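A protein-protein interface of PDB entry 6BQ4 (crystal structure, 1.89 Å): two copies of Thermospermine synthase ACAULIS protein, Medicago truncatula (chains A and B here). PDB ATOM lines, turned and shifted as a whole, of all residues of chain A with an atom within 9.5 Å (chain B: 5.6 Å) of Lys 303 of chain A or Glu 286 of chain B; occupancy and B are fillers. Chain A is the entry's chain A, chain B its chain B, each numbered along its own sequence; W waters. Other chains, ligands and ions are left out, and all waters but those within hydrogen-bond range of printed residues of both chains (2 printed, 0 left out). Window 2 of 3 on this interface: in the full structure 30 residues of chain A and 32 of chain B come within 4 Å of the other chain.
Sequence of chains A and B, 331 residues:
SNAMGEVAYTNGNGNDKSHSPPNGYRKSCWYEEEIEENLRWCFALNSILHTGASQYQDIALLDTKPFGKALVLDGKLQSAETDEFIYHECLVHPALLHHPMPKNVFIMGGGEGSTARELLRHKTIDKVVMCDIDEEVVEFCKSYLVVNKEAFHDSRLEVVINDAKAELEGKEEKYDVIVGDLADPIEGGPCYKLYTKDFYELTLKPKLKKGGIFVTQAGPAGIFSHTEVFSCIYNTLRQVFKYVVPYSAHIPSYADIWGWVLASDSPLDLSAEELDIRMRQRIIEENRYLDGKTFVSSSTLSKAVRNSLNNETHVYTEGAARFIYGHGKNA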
ATOM      1  N   ILE A 223       8.704  -9.907   9.903  1.00  0.00           N
ATOM      2  CA  ILE A 223       9.474 -10.232  11.060  1.00  0.00           C
ATOM      3  C   ILE A 223      11.014 -10.092  10.868  1.00  0.00           C
ATOM      4  O   ILE A 223      11.690  -9.623  11.780  1.00  0.00           O
ATOM      5  CB  ILE A 223       9.051 -11.585  11.597  1.00  0.00           C
ATOM      6  CG1 ILE A 223       9.742 -11.941  12.908  1.00  0.00           C
ATOM      7  CG2 ILE A 223       9.313 -12.667  10.555  1.00  0.00           C
ATOM      8  CD1 ILE A 223       9.219 -11.171  14.073  1.00  0.00           C
ATOM      9  N   HIS A 226      11.757  -6.298   8.178  1.00  0.00           N
ATOM     10  CA  HIS A 226      11.578  -4.926   8.746  1.00  0.00           C
ATOM     11  C   HIS A 226      12.875  -4.184   9.057  1.00  0.00           C
ATOM     12  O   HIS A 226      12.841  -2.975   9.234  1.00  0.00           O
ATOM     13  CB  HIS A 226      10.717  -4.888  10.015  1.00  0.00           C
ATOM     14  CG  HIS A 226      11.405  -5.446  11.213  1.00  0.00           C
ATOM     15  ND1 HIS A 226      11.523  -6.801  11.432  1.00  0.00           N
ATOM     16  CD2 HIS A 226      12.137  -4.833  12.177  1.00  0.00           C
ATOM     17  CE1 HIS A 226      12.226  -6.989  12.545  1.00  0.00           C
ATOM     18  NE2 HIS A 226      12.620  -5.818  12.999  1.00  0.00           N
ATOM     19  N   THR A 300      -0.152  -1.557  16.119  1.00  0.00           N
ATOM     20  CA  THR A 300       0.394  -2.359  17.209  1.00  0.00           C
ATOM     21  C   THR A 300       1.335  -3.424  16.608  1.00  0.00           C
ATOM     22  O   THR A 300       0.910  -4.476  16.192  1.00  0.00           O
ATOM     23  CB  THR A 300      -0.730  -3.085  17.969  1.00  0.00           C
ATOM     24  OG1 THR A 300      -1.789  -2.184  18.302  1.00  0.00           O
ATOM     25  CG2 THR A 300      -0.187  -3.780  19.276  1.00  0.00           C
ATOM     26  N   LEU A 301       2.613  -3.141  16.591  1.00  0.00           N
ATOM     27  CA  LEU A 301       3.572  -3.986  15.963  1.00  0.00           C
ATOM     28  C   LEU A 301       3.912  -5.133  16.881  1.00  0.00           C
ATOM     29  O   LEU A 301       3.613  -5.061  18.075  1.00  0.00           O
ATOM     30  CB  LEU A 301       4.842  -3.194  15.685  1.00  0.00           C
ATOM     31  CG  LEU A 301       4.558  -1.941  14.846  1.00  0.00           C
ATOM     32  CD1 LEU A 301       5.827  -1.131  14.693  1.00  0.00           C
ATOM     33  CD2 LEU A 301       3.997  -2.332  13.498  1.00  0.00           C
ATOM     34  N   SER A 302       4.521  -6.170  16.325  1.00  0.00           N
ATOM     35  CA  SER A 302       4.902  -7.339  17.121  1.00  0.00           C
ATOM     36  C   SER A 302       6.172  -7.059  17.931  1.00  0.00           C
ATOM     37  O   SER A 302       6.879  -6.045  17.715  1.00  0.00           O
ATOM     38  CB  SER A 302       5.046  -8.594  16.252  1.00  0.00           C
ATOM     39  OG  SER A 302       6.258  -8.598  15.525  1.00  0.00           O
ATOM     40  N   LYS A 303       6.423  -7.960  18.865  1.00  0.00           N
ATOM     41  CA  LYS A 303       7.496  -7.837  19.825  1.00  0.00           C
ATOM     42  C   LYS A 303       8.831  -7.496  19.179  1.00  0.00           C
ATOM     43  O   LYS A 303       9.442  -6.503  19.564  1.00  0.00           O
ATOM     44  CB  LYS A 303       7.710  -9.143  20.611  1.00  0.00           C
ATOM     45  CG  LYS A 303       8.813  -8.983  21.645  1.00  0.00           C
ATOM     46  CD  LYS A 303       8.930 -10.236  22.461  1.00  0.00           C
ATOM     47  CE  LYS A 303       9.664  -9.934  23.754  1.00  0.00           C
ATOM     48  NZ  LYS A 303      10.069 -11.221  24.374  1.00  0.00           N
ATOM     49  N   ALA A 304       9.285  -8.327  18.242  1.00  0.00           N
ATOM     50  CA  ALA A 304      10.602  -8.160  17.669  1.00  0.00           C
ATOM     51  C   ALA A 304      10.670  -6.894  16.772  1.00  0.00           C
ATOM     52  O   ALA A 304      11.660  -6.190  16.747  1.00  0.00           O
ATOM     53  CB  ALA A 304      11.006  -9.404  16.908  1.00  0.00           C
ATOM     54  N   VAL A 305       9.567  -6.566  16.112  1.00  0.00           N
ATOM     55  CA  VAL A 305       9.539  -5.387  15.276  1.00  0.00           C
ATOM     56  C   VAL A 305       9.567  -4.094  16.143  1.00  0.00           C
ATOM     57  O   VAL A 305      10.378  -3.198  15.879  1.00  0.00           O
ATOM     58  CB  VAL A 305       8.332  -5.414  14.307  1.00  0.00           C
ATOM     59  CG1 VAL A 305       8.342  -4.172  13.418  1.00  0.00           C
ATOM     60  CG2 VAL A 305       8.349  -6.663  13.446  1.00  0.00           C
ATOM     61  N   ARG A 306       8.710  -4.017  17.172  1.00  0.00           N
ATOM     62  CA  ARG A 306       8.710  -2.897  18.105  1.00  0.00           C
ATOM     63  C   ARG A 306      10.092  -2.702  18.724  1.00  0.00           C
ATOM     64  O   ARG A 306      10.567  -1.568  18.814  1.00  0.00           O
ATOM     65  CB  ARG A 306       7.735  -3.127  19.239  1.00  0.00           C
ATOM     66  CG  ARG A 306       6.789  -2.012  19.507  1.00  0.00           C
ATOM     67  CD  ARG A 306       5.884  -2.390  20.641  1.00  0.00           C
ATOM     68  NE  ARG A 306       5.161  -3.620  20.330  1.00  0.00           N
ATOM     69  CZ  ARG A 306       5.144  -4.709  21.111  1.00  0.00           C
ATOM     70  NH1 ARG A 306       5.790  -4.711  22.283  1.00  0.00           N
ATOM     71  NH2 ARG A 306       4.457  -5.794  20.732  1.00  0.00           N
ATOM     72  N   ASN A 307      10.716  -3.803  19.170  1.00  0.00           N
ATOM     73  CA  ASN A 307      12.066  -3.773  19.734  1.00  0.00           C
ATOM     74  C   ASN A 307      13.063  -3.183  18.782  1.00  0.00           C
ATOM     75  O   ASN A 307      13.818  -2.305  19.190  1.00  0.00           O
ATOM     76  CB  ASN A 307      12.555  -5.162  20.152  1.00  0.00           C
ATOM     77  CG  ASN A 307      12.168  -5.498  21.556  1.00  0.00           C
ATOM     78  OD1 ASN A 307      11.767  -4.624  22.297  1.00  0.00           O
ATOM     79  ND2 ASN A 307      12.300  -6.758  21.947  1.00  0.00           N
ATOM     80  N   SER A 308      13.092  -3.664  17.543  1.00  0.00           N
ATOM     81  CA  SER A 308      13.988  -3.082  16.518  1.00  0.00           C
ATOM     82  C   SER A 308      13.807  -1.579  16.312  1.00  0.00           C
ATOM     83  O   SER A 308      14.758  -0.800  16.357  1.00  0.00           O
ATOM     84  CB  SER A 308      13.800  -3.730  15.185  1.00  0.00           C
ATOM     85  OG  SER A 308      14.398  -4.973  15.142  1.00  0.00           O
ATOM     86  N   LEU A 309      12.563  -1.183  16.126  1.00  0.00           N
ATOM     87  CA  LEU A 309      12.224   0.222  16.009  1.00  0.00           C
ATOM     88  C   LEU A 309      12.672   1.030  17.208  1.00  0.00           C
ATOM     89  O   LEU A 309      13.358   2.041  17.042  1.00  0.00           O
ATOM     90  CB  LEU A 309      10.725   0.426  15.748  1.00  0.00           C
ATOM     91  CG  LEU A 309      10.454   0.482  14.243  1.00  0.00           C
ATOM     92  CD1 LEU A 309      10.850  -0.791  13.515  1.00  0.00           C
ATOM     93  CD2 LEU A 309       9.004   0.907  13.933  1.00  0.00           C
ATOM     94  N   ASN A 310      12.306   0.591  18.407  1.00  0.00           N
ATOM     95  CA  ASN A 310      12.648   1.349  19.604  1.00  0.00           C
ATOM     96  C   ASN A 310      14.183   1.362  19.871  1.00  0.00           C
ATOM     97  O   ASN A 310      14.669   2.340  20.441  1.00  0.00           O
ATOM     98  CB  ASN A 310      11.818   0.897  20.839  1.00  0.00           C
ATOM     99  CG  ASN A 310      10.313   1.274  20.742  1.00  0.00           C
ATOM    100  OD1 ASN A 310       9.509   0.830  21.561  1.00  0.00           O
ATOM    101  ND2 ASN A 310       9.935   2.082  19.747  1.00  0.00           N
ATOM    102  N   ASN A 311      14.920   0.402  19.352  1.00  0.00           N
ATOM    103  CA  ASN A 311      16.335   0.358  19.572  1.00  0.00           C
ATOM    104  C   ASN A 311      17.181   0.761  18.390  1.00  0.00           C
ATOM    105  O   ASN A 311      18.383   0.694  18.446  1.00  0.00           O
ATOM    106  CB  ASN A 311      16.745  -1.048  19.952  1.00  0.00           C
ATOM    107  CG  ASN A 311      16.136  -1.507  21.253  1.00  0.00           C
ATOM    108  OD1 ASN A 311      15.786  -0.708  22.093  1.00  0.00           O
ATOM    109  ND2 ASN A 311      16.000  -2.804  21.414  1.00  0.00           N
ATOM    110  N   GLU B  89       4.700 -20.580  19.007  1.00  0.00           N
ATOM    111  CA  GLU B  89       4.374 -19.653  20.103  1.00  0.00           C
ATOM    112  C   GLU B  89       2.918 -19.216  20.053  1.00  0.00           C
ATOM    113  O   GLU B  89       2.310 -19.107  21.100  1.00  0.00           O
ATOM    114  CB  GLU B  89       5.284 -18.404  20.127  1.00  0.00           C
ATOM    115  CG  GLU B  89       6.727 -18.715  20.574  1.00  0.00           C
ATOM    116  CD  GLU B  89       7.620 -17.461  20.695  1.00  0.00           C
ATOM    117  OE1 GLU B  89       7.079 -16.358  20.673  1.00  0.00           O
ATOM    118  OE2 GLU B  89       8.883 -17.592  20.785  1.00  0.00           O
ATOM    119  N   ARG B 121       8.012 -25.291  28.105  1.00  0.00           N
ATOM    120  CA  ARG B 121       8.591 -24.085  28.629  1.00  0.00           C
ATOM    121  C   ARG B 121       7.739 -23.505  29.746  1.00  0.00           C
ATOM    122  O   ARG B 121       8.207 -22.617  30.452  1.00  0.00           O
ATOM    123  CB  ARG B 121       8.780 -23.012  27.502  1.00  0.00           C
ATOM    124  CG  ARG B 121       9.836 -23.323  26.474  1.00  0.00           C
ATOM    125  CD  ARG B 121       9.758 -22.310  25.319  1.00  0.00           C
ATOM    126  NE  ARG B 121      10.041 -21.029  25.902  1.00  0.00           N
ATOM    127  CZ  ARG B 121       9.754 -19.862  25.342  1.00  0.00           C
ATOM    128  NH1 ARG B 121       9.150 -19.814  24.143  1.00  0.00           N
ATOM    129  NH2 ARG B 121      10.057 -18.734  25.975  1.00  0.00           N
ATOM    130  N   ARG B 280       6.442 -13.713  31.965  1.00  0.00           N
ATOM    131  CA  ARG B 280       7.606 -13.499  32.830  1.00  0.00           C
ATOM    132  C   ARG B 280       7.641 -14.498  33.990  1.00  0.00           C
ATOM    133  O   ARG B 280       8.679 -15.044  34.288  1.00  0.00           O
ATOM    134  CB  ARG B 280       7.544 -12.069  33.376  1.00  0.00           C
ATOM    135  CG  ARG B 280       8.708 -11.632  34.279  1.00  0.00           C
ATOM    136  CD  ARG B 280      10.013 -11.439  33.513  1.00  0.00           C
ATOM    137  NE  ARG B 280       9.860 -10.503  32.389  1.00  0.00           N
ATOM    138  CZ  ARG B 280      10.016  -9.176  32.477  1.00  0.00           C
ATOM    139  NH1 ARG B 280      10.362  -8.610  33.644  1.00  0.00           N
ATOM    140  NH2 ARG B 280       9.836  -8.412  31.398  1.00  0.00           N
ATOM    141  N   ILE B 284       9.732 -20.361  30.798  1.00  0.00           N
ATOM    142  CA  ILE B 284      11.202 -20.324  30.815  1.00  0.00           C
ATOM    143  C   ILE B 284      11.708 -19.737  29.481  1.00  0.00           C
ATOM    144  O   ILE B 284      11.241 -20.095  28.381  1.00  0.00           O
ATOM    145  CB  ILE B 284      11.863 -21.694  31.093  1.00  0.00           C
ATOM    146  CG1 ILE B 284      11.148 -22.470  32.204  1.00  0.00           C
ATOM    147  CG2 ILE B 284      13.313 -21.486  31.554  1.00  0.00           C
ATOM    148  CD1 ILE B 284      11.822 -23.799  32.567  1.00  0.00           C
ATOM    149  N   GLU B 285      12.674 -18.836  29.598  1.00  0.00           N
ATOM    150  CA  GLU B 285      13.243 -18.131  28.464  1.00  0.00           C
ATOM    151  C   GLU B 285      12.254 -17.086  27.899  1.00  0.00           C
ATOM    152  O   GLU B 285      11.078 -17.081  28.202  1.00  0.00           O
ATOM    153  CB  GLU B 285      13.786 -19.126  27.378  1.00  0.00           C
ATOM    154  CG  GLU B 285      14.743 -20.245  27.899  1.00  0.00           C
ATOM    155  CD  GLU B 285      14.729 -21.588  27.099  1.00  0.00           C
ATOM    156  OE1 GLU B 285      15.050 -22.657  27.697  1.00  0.00           O
ATOM    157  OE2 GLU B 285      14.420 -21.571  25.882  1.00  0.00           O
ATOM    158  N   GLU B 286      12.770 -16.188  27.090  1.00  0.00           N
ATOM    159  CA  GLU B 286      12.019 -15.120  26.474  1.00  0.00           C
ATOM    160  C   GLU B 286      11.290 -15.585  25.207  1.00  0.00           C
ATOM    161  O   GLU B 286      11.906 -16.167  24.337  1.00  0.00           O
ATOM    162  CB  GLU B 286      13.019 -14.064  26.001  1.00  0.00           C
ATOM    163  CG  GLU B 286      13.503 -13.125  27.076  1.00  0.00           C
ATOM    164  CD  GLU B 286      12.692 -11.838  27.086  1.00  0.00           C
ATOM    165  OE1 GLU B 286      12.262 -11.419  28.197  1.00  0.00           O
ATOM    166  OE2 GLU B 286      12.483 -11.238  25.971  1.00  0.00           O
ATOM    167  N   ASN B 287      10.012 -15.324  25.046  1.00  0.00           N
ATOM    168  CA  ASN B 287       9.419 -15.593  23.728  1.00  0.00           C
ATOM    169  C   ASN B 287      10.170 -14.765  22.646  1.00  0.00           C
ATOM    170  O   ASN B 287      10.686 -13.672  22.945  1.00  0.00           O
ATOM    171  CB  ASN B 287       7.964 -15.229  23.726  1.00  0.00           C
ATOM    172  CG  ASN B 287       7.124 -16.218  24.484  1.00  0.00           C
ATOM    173  OD1 ASN B 287       7.599 -17.263  24.946  1.00  0.00           O
ATOM    174  ND2 ASN B 287       5.885 -15.848  24.703  1.00  0.00           N
ATOM    175  N   ARG B 288      10.265 -15.313  21.430  1.00  0.00           N
ATOM    176  CA  ARG B 288      10.884 -14.598  20.334  1.00  0.00           C
ATOM    177  C   ARG B 288       9.865 -13.798  19.542  1.00  0.00           C
ATOM    178  O   ARG B 288      10.188 -12.760  18.986  1.00  0.00           O
ATOM    179  CB  ARG B 288      11.654 -15.583  19.460  1.00  0.00           C
ATOM    180  CG  ARG B 288      12.825 -16.218  20.233  1.00  0.00           C
ATOM    181  CD  ARG B 288      13.877 -16.785  19.324  1.00  0.00           C
ATOM    182  NE  ARG B 288      13.626 -18.141  18.830  1.00  0.00           N
ATOM    183  CZ  ARG B 288      14.056 -18.609  17.641  1.00  0.00           C
ATOM    184  NH1 ARG B 288      13.817 -19.865  17.295  1.00  0.00           N
ATOM    185  NH2 ARG B 288      14.722 -17.809  16.803  1.00  0.00           N
ATOM    186  N   TYR B 289       8.617 -14.255  19.492  1.00  0.00           N
ATOM    187  CA  TYR B 289       7.618 -13.583  18.626  1.00  0.00           C
ATOM    188  C   TYR B 289       6.616 -12.886  19.505  1.00  0.00           C
ATOM    189  O   TYR B 289       6.264 -11.727  19.271  1.00  0.00           O
ATOM    190  CB  TYR B 289       6.898 -14.569  17.724  1.00  0.00           C
ATOM    191  CG  TYR B 289       5.828 -13.873  16.937  1.00  0.00           C
ATOM    192  CD1 TYR B 289       6.178 -13.015  15.917  1.00  0.00           C
ATOM    193  CD2 TYR B 289       4.468 -14.024  17.258  1.00  0.00           C
ATOM    194  CE1 TYR B 289       5.214 -12.358  15.214  1.00  0.00           C
ATOM    195  CE2 TYR B 289       3.511 -13.351  16.552  1.00  0.00           C
ATOM    196  CZ  TYR B 289       3.896 -12.511  15.567  1.00  0.00           C
ATOM    197  OH  TYR B 289       2.978 -11.803  14.857  1.00  0.00           O
ATOM    198  N   LEU B 290       6.126 -13.607  20.521  1.00  0.00           N
ATOM    199  CA  LEU B 290       4.907 -13.191  21.223  1.00  0.00           C
ATOM    200  C   LEU B 290       5.191 -12.423  22.489  1.00  0.00           C
ATOM    201  O   LEU B 290       5.818 -12.948  23.409  1.00  0.00           O
ATOM    202  CB  LEU B 290       4.053 -14.428  21.585  1.00  0.00           C
ATOM    203  CG  LEU B 290       2.570 -14.159  21.945  1.00  0.00           C
ATOM    204  CD1 LEU B 290       1.664 -13.898  20.739  1.00  0.00           C
ATOM    205  CD2 LEU B 290       2.030 -15.322  22.754  1.00  0.00           C
ATOM    206  N   ASP B 291       4.713 -11.188  22.558  1.00  0.00           N
ATOM    207  CA  ASP B 291       4.431 -10.490  23.858  1.00  0.00           C
ATOM    208  C   ASP B 291       2.951 -10.175  23.914  1.00  0.00           C
ATOM    209  O   ASP B 291       2.198 -10.576  23.042  1.00  0.00           O
ATOM    210  CB  ASP B 291       5.350  -9.285  24.091  1.00  0.00           C
ATOM    211  CG  ASP B 291       5.146  -8.168  23.100  1.00  0.00           C
ATOM    212  OD1 ASP B 291       4.200  -8.262  22.283  1.00  0.00           O
ATOM    213  OD2 ASP B 291       5.956  -7.182  23.133  1.00  0.00           O
ATOM    214  N   THR B 294       1.549  -8.046  21.130  1.00  0.00           N
ATOM    215  CA  THR B 294       1.486  -8.809  19.890  1.00  0.00           C
ATOM    216  C   THR B 294       0.218  -9.667  19.902  1.00  0.00           C
ATOM    217  O   THR B 294      -0.455  -9.769  18.885  1.00  0.00           O
ATOM    218  CB  THR B 294       2.717  -9.709  19.717  1.00  0.00           C
ATOM    219  OG1 THR B 294       3.916  -8.941  19.805  1.00  0.00           O
ATOM    220  CG2 THR B 294       2.692 -10.454  18.387  1.00  0.00           C
HETATM  221  O   HOH W   1       7.653 -10.454  17.296  1.00  0.00           O
HETATM  222  O   HOH W   2       7.471 -11.835  25.458  1.00  0.00           O
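The side-chain amino group of Lys 303 of chain A lies within salt-bridge range of the side-chain carboxylate of Glu 286 of chain B (2.9 Å). NZ of Lys 303 of chain A sits at hydrogen-bond distance from O of Asn 287 of chain B (2.9 Å). The backbone NH (N) of Lys 303 of chain A sits at hydrogen-bond distance from the side-chain hydroxyl (OG1) of Thr 294 of chain B (2.9 Å). The guanidinium group of Arg 306 of chain A lies within salt-bridge range of the side-chain carboxylate of Asp 291 of chain B. OG1 of Thr 294 of chain B sits at hydrogen-bond distance from NH2 of Arg 306 of chain A (3.3 Å).
NH2 of Arg 306 of chain A lies within hydrogen-bond range of O of Leu 301 of chain A. N of Tyr 289 of chain B lies within hydrogen-bond range of OE1 of Glu 89 of chain B (2.9 Å). NH2 of Arg 121 of chain B sits at hydrogen-bond distance from OD1 of Asn 287 of chain B, at 3.0 Å. O of Leu 290 of chain B sits close to ND2 of Asn 287 of chain B (3.2 Å). The side-chain hydroxyl of Thr 294 of chain B is in hydrogen-bond range of the side-chain carboxylate of Asp 291 of chain B (2.6 Å).
Among the printed residues, pairs that only touch across the chains: Lys 303 of chain A with Tyr 289 of chain B (3.3 Å), Ser 302 of chain A with Thr 294 of chain B (3.3 Å), Lys 303 of chain A with Asp 291 of chain B (3.6 Å) and Ser 302 of chain A with Tyr 289 of chain B (3.9 Å).
Lys 303 of chain A touches just these residues of chain B: Glu 286 (2.9 Å), Asn 287 (2.9 Å), Tyr 289 (3.3 Å), Asp 291 (3.6 Å) and Thr 294 (2.9 Å). Asn 287 of chain B touches just one residue of chain A: Lys 303. Of the printed residues of chain B, Ser 302 of chain A touches Tyr 289 and Thr 294. Printed residues of chain B within 4 Å of Arg 306 of chain A: Asp 291 (2.6 Å) and Thr 294 (3.3 Å). The nearest residue of chain B that does not touch Lys 303 of chain A is Leu 290 of chain B (4.2 Å). The nearest residue of chain A that does not touch Glu 286 of chain B is Asn 307 of chain A (6.0 Å).
Of the 12 printed residues of chain B, 5 touch a printed residue of chain A. Hydrophobic or aromatic side chains of chain B within 4 Å of the printed part of chain A: Tyr 289. Printed residues of chain A that touch a printed residue of chain B: Ser 302, Lys 303 and Arg 306. Among the printed residues, Asp or Glu carboxylates within 4 Å of a Lys or Arg side-chain nitrogen of the other chain: Lys 303 of chain A with Glu 286 of chain B (2.9 Å) and Arg 306 of chain A with Asp 291 of chain B (2.6 Å).
No position is printed for both chains.
Water W1 lies within hydrogen-bond range of O of Tyr 289 of chain B, N of Ala 304 of chain A, OG of Ser 302 of chain A and N of Lys 303 of chain A. Water W2 lies within hydrogen-bond range of O of Leu 290 of chain B (2.9 Å) and NZ of Lys 303 of chain A (2.9 Å).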
